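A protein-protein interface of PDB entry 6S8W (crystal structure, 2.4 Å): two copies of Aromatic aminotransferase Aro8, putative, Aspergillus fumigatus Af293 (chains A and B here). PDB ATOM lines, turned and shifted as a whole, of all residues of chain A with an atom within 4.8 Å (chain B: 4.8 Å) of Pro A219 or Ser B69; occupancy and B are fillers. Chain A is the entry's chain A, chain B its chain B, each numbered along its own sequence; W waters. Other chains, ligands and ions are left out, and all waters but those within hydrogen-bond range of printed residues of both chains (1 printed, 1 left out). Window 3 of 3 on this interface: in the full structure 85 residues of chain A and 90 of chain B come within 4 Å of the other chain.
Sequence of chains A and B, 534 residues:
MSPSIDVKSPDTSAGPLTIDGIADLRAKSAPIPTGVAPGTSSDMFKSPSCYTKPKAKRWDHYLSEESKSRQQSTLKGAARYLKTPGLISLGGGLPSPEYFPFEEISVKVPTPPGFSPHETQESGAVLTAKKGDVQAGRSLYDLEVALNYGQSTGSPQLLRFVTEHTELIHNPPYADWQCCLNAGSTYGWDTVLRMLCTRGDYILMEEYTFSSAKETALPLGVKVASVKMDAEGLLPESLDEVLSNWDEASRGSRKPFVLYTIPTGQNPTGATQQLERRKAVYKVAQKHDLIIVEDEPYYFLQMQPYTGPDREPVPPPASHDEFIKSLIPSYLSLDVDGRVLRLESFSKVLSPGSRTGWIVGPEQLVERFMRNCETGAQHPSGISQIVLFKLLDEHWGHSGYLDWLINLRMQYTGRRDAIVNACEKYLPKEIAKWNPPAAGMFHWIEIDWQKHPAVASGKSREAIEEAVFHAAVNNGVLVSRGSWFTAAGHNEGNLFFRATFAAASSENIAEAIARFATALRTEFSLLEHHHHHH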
ATOM      1  N   ARG A 199      18.264  21.586  -6.669  1.00  0.00           N
ATOM      2  CA  ARG A 199      17.063  21.186  -7.442  1.00  0.00           C
ATOM      3  C   ARG A 199      16.416  22.421  -8.067  1.00  0.00           C
ATOM      4  O   ARG A 199      16.116  23.367  -7.368  1.00  0.00           O
ATOM      5  CB  ARG A 199      16.033  20.475  -6.562  1.00  0.00           C
ATOM      6  CG  ARG A 199      16.431  19.077  -6.136  1.00  0.00           C
ATOM      7  CD  ARG A 199      15.254  18.167  -5.885  1.00  0.00           C
ATOM      8  NE  ARG A 199      14.803  17.480  -7.076  1.00  0.00           N
ATOM      9  CZ  ARG A 199      15.296  16.337  -7.498  1.00  0.00           C
ATOM     10  NH1 ARG A 199      16.261  15.752  -6.823  1.00  0.00           N
ATOM     11  NH2 ARG A 199      14.824  15.781  -8.587  1.00  0.00           N
ATOM     12  N   GLU A 215      23.288  12.287 -17.557  1.00  0.00           N
ATOM     13  CA  GLU A 215      22.552  11.301 -16.721  1.00  0.00           C
ATOM     14  C   GLU A 215      22.937  11.463 -15.247  1.00  0.00           C
ATOM     15  O   GLU A 215      22.135  11.048 -14.388  1.00  0.00           O
ATOM     16  CB  GLU A 215      22.841   9.872 -17.180  1.00  0.00           C
ATOM     17  CG  GLU A 215      21.965   9.423 -18.331  1.00  0.00           C
ATOM     18  CD  GLU A 215      22.570   8.321 -19.181  1.00  0.00           C
ATOM     19  OE1 GLU A 215      23.490   7.637 -18.691  1.00  0.00           O
ATOM     20  OE2 GLU A 215      22.126   8.154 -20.336  1.00  0.00           O
ATOM     21  N   THR A 216      24.116  12.025 -14.966  1.00  0.00           N
ATOM     22  CA  THR A 216      24.601  12.277 -13.583  1.00  0.00           C
ATOM     23  C   THR A 216      23.839  13.463 -12.992  1.00  0.00           C
ATOM     24  O   THR A 216      23.751  13.547 -11.751  1.00  0.00           O
ATOM     25  CB  THR A 216      26.110  12.548 -13.534  1.00  0.00           C
ATOM     26  OG1 THR A 216      26.803  11.345 -13.869  1.00  0.00           O
ATOM     27  CG2 THR A 216      26.564  13.033 -12.175  1.00  0.00           C
ATOM     28  N   ALA A 217      23.300  14.338 -13.851  1.00  0.00           N
ATOM     29  CA  ALA A 217      22.714  15.638 -13.460  1.00  0.00           C
ATOM     30  C   ALA A 217      21.182  15.564 -13.427  1.00  0.00           C
ATOM     31  O   ALA A 217      20.595  16.212 -12.540  1.00  0.00           O
ATOM     32  CB  ALA A 217      23.193  16.723 -14.394  1.00  0.00           C
ATOM     33  N   LEU A 218      20.549  14.821 -14.343  1.00  0.00           N
ATOM     34  CA  LEU A 218      19.068  14.829 -14.504  1.00  0.00           C
ATOM     35  C   LEU A 218      18.399  14.418 -13.191  1.00  0.00           C
ATOM     36  O   LEU A 218      17.479  15.098 -12.743  1.00  0.00           O
ATOM     37  CB  LEU A 218      18.656  13.929 -15.674  1.00  0.00           C
ATOM     38  CG  LEU A 218      18.946  14.509 -17.059  1.00  0.00           C
ATOM     39  CD1 LEU A 218      18.161  13.780 -18.140  1.00  0.00           C
ATOM     40  CD2 LEU A 218      18.637  15.998 -17.097  1.00  0.00           C
ATOM     41  N   PRO A 219      18.820  13.320 -12.520  1.00  0.00           N
ATOM     42  CA  PRO A 219      18.160  12.886 -11.286  1.00  0.00           C
ATOM     43  C   PRO A 219      18.364  13.805 -10.070  1.00  0.00           C
ATOM     44  O   PRO A 219      17.679  13.603  -9.084  1.00  0.00           O
ATOM     45  CB  PRO A 219      18.774  11.505 -11.006  1.00  0.00           C
ATOM     46  CG  PRO A 219      20.115  11.534 -11.711  1.00  0.00           C
ATOM     47  CD  PRO A 219      19.910  12.418 -12.925  1.00  0.00           C
ATOM     48  N   LEU A 220      19.276  14.778 -10.158  1.00  0.00           N
ATOM     49  CA  LEU A 220      19.526  15.776  -9.081  1.00  0.00           C
ATOM     50  C   LEU A 220      18.569  16.958  -9.264  1.00  0.00           C
ATOM     51  O   LEU A 220      18.654  17.919  -8.473  1.00  0.00           O
ATOM     52  CB  LEU A 220      20.988  16.229  -9.134  1.00  0.00           C
ATOM     53  CG  LEU A 220      22.014  15.145  -8.808  1.00  0.00           C
ATOM     54  CD1 LEU A 220      23.431  15.671  -8.973  1.00  0.00           C
ATOM     55  CD2 LEU A 220      21.802  14.607  -7.401  1.00  0.00           C
ATOM     56  N   GLY A 221      17.694  16.874 -10.269  1.00  0.00           N
ATOM     57  CA  GLY A 221      16.702  17.916 -10.600  1.00  0.00           C
ATOM     58  C   GLY A 221      17.332  19.055 -11.379  1.00  0.00           C
ATOM     59  O   GLY A 221      16.675  20.105 -11.530  1.00  0.00           O
ATOM     60  N   GLU B  65      12.905  11.160  -4.676  1.00  0.00           N
ATOM     61  CA  GLU B  65      12.569  11.645  -6.039  1.00  0.00           C
ATOM     62  C   GLU B  65      13.835  11.586  -6.899  1.00  0.00           C
ATOM     63  O   GLU B  65      13.725  11.261  -8.098  1.00  0.00           O
ATOM     64  CB  GLU B  65      11.988  13.058  -5.970  1.00  0.00           C
ATOM     65  CG  GLU B  65      11.742  13.681  -7.331  1.00  0.00           C
ATOM     66  N   GLU B  66      14.986  11.893  -6.294  1.00  0.00           N
ATOM     67  CA  GLU B  66      16.334  11.669  -6.878  1.00  0.00           C
ATOM     68  C   GLU B  66      16.412  10.226  -7.390  1.00  0.00           C
ATOM     69  O   GLU B  66      16.591  10.036  -8.611  1.00  0.00           O
ATOM     70  CB  GLU B  66      17.413  11.925  -5.822  1.00  0.00           C
ATOM     71  CG  GLU B  66      18.799  12.139  -6.403  1.00  0.00           C
ATOM     72  CD  GLU B  66      19.927  12.159  -5.384  1.00  0.00           C
ATOM     73  OE1 GLU B  66      19.842  12.953  -4.426  1.00  0.00           O
ATOM     74  OE2 GLU B  66      20.884  11.376  -5.549  1.00  0.00           O
ATOM     75  N   SER B  67      16.264   9.259  -6.480  1.00  0.00           N
ATOM     76  CA  SER B  67      16.461   7.805  -6.715  1.00  0.00           C
ATOM     77  C   SER B  67      15.504   7.296  -7.803  1.00  0.00           C
ATOM     78  O   SER B  67      15.961   6.521  -8.667  1.00  0.00           O
ATOM     79  CB  SER B  67      16.304   7.030  -5.431  1.00  0.00           C
ATOM     80  OG  SER B  67      16.695   5.677  -5.605  1.00  0.00           O
ATOM     81  N   LYS B  68      14.231   7.708  -7.763  1.00  0.00           N
ATOM     82  CA  LYS B  68      13.197   7.289  -8.751  1.00  0.00           C
ATOM     83  C   LYS B  68      13.536   7.871 -10.128  1.00  0.00           C
ATOM     84  O   LYS B  68      13.206   7.216 -11.136  1.00  0.00           O
ATOM     85  CB  LYS B  68      11.793   7.723  -8.312  1.00  0.00           C
ATOM     86  CG  LYS B  68      10.967   6.633  -7.641  1.00  0.00           C
ATOM     87  CD  LYS B  68       9.586   7.081  -7.214  1.00  0.00           C
ATOM     88  CE  LYS B  68       8.673   5.919  -6.878  1.00  0.00           C
ATOM     89  NZ  LYS B  68       7.307   6.375  -6.526  1.00  0.00           N
ATOM     90  N   SER B  69      14.165   9.049 -10.167  1.00  0.00           N
ATOM     91  CA  SER B  69      14.537   9.767 -11.415  1.00  0.00           C
ATOM     92  C   SER B  69      15.645   9.012 -12.159  1.00  0.00           C
ATOM     93  O   SER B  69      15.674   9.099 -13.402  1.00  0.00           O
ATOM     94  CB  SER B  69      14.953  11.187 -11.128  1.00  0.00           C
ATOM     95  OG  SER B  69      13.838  12.063 -11.192  1.00  0.00           O
ATOM     96  N   ARG B  70      16.518   8.311 -11.428  1.00  0.00           N
ATOM     97  CA  ARG B  70      17.727   7.655 -11.996  1.00  0.00           C
ATOM     98  C   ARG B  70      17.287   6.618 -13.033  1.00  0.00           C
ATOM     99  O   ARG B  70      16.224   5.997 -12.843  1.00  0.00           O
ATOM    100  CB  ARG B  70      18.581   7.028 -10.890  1.00  0.00           C
ATOM    101  CG  ARG B  70      18.835   7.957  -9.712  1.00  0.00           C
ATOM    102  CD  ARG B  70      20.158   7.680  -9.025  1.00  0.00           C
ATOM    103  NE  ARG B  70      21.219   8.514  -9.569  1.00  0.00           N
ATOM    104  CZ  ARG B  70      21.876   9.441  -8.882  1.00  0.00           C
ATOM    105  NH1 ARG B  70      21.597   9.644  -7.605  1.00  0.00           N
ATOM    106  NH2 ARG B  70      22.820  10.154  -9.471  1.00  0.00           N
ATOM    107  N   GLN B  71      18.089   6.454 -14.087  1.00  0.00           N
ATOM    108  CA  GLN B  71      17.795   5.574 -15.247  1.00  0.00           C
ATOM    109  C   GLN B  71      19.080   4.865 -15.681  1.00  0.00           C
ATOM    110  O   GLN B  71      20.164   5.284 -15.229  1.00  0.00           O
ATOM    111  CB  GLN B  71      17.243   6.404 -16.406  1.00  0.00           C
ATOM    112  CG  GLN B  71      18.246   7.413 -16.949  1.00  0.00           C
ATOM    113  CD  GLN B  71      17.694   8.228 -18.092  1.00  0.00           C
ATOM    114  OE1 GLN B  71      16.482   8.333 -18.277  1.00  0.00           O
ATOM    115  NE2 GLN B  71      18.585   8.818 -18.871  1.00  0.00           N
HETATM  116  O   HOH W   1      20.587   8.082 -13.956  1.00  0.00           O
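Along chain B the printed residues that touch a printed residue of chain A span positions 65 to 71. Printed residues of chain A that touch a printed residue of chain B: Arg A199, Glu A215, Pro A219 and Leu A220. Hydrophobic or aromatic side chains of chain A within 4 Å of the printed part of chain B: Pro A219 and Leu A220. Among the printed residues, no Asp or Glu carboxylate lies within 4 Å of a Lys or Arg side-chain nitrogen of the other chain.
No position is printed for both chains. Of the 6 pairs that touch across the chains among the printed residues, none has its exchanged pair printed and touching as well.
Water W1 bridges the backbone NH (N) of Gln B71 (3.0 Å) and the backbone carbonyl oxygen (O) of Glu A215 (3.4 Å).
Among the printed residues, pairs that only touch across the chains: Arg A199 with Glu B65, Glu A215 with Gln B71, Pro A219 with Glu B66, Pro A219 with Ser B69, Pro A219 with Arg B70 and Leu A220 with Glu B66.
The side-chain hydroxyl of Ser B69 is in hydrogen-bond range of the backbone carbonyl oxygen of Glu B65 (3.2 Å). The backbone carbonyl oxygen of Pro A219 is in hydrogen-bond range of the guanidinium group of Arg A199 (3.4 Å). OE2 of Glu B66 lies within salt-bridge range of NH1 of Arg B70.
Pro A219 touches just these residues of chain B: Glu B66, Ser B69 and Arg B70. Printed residues of chain B within 4 Å of Leu A220: Glu B66 (3.7 Å). Of the printed residues of chain A, Glu B65 touches Arg A199. Ser B69 touches one residue of chain A. The nearest residue of chain B that does not touch Pro A219 is Glu B65 (4.7 Å). The nearest printed residue of chain B that does not touch Glu A215 is Arg B70 (5.0 Å).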
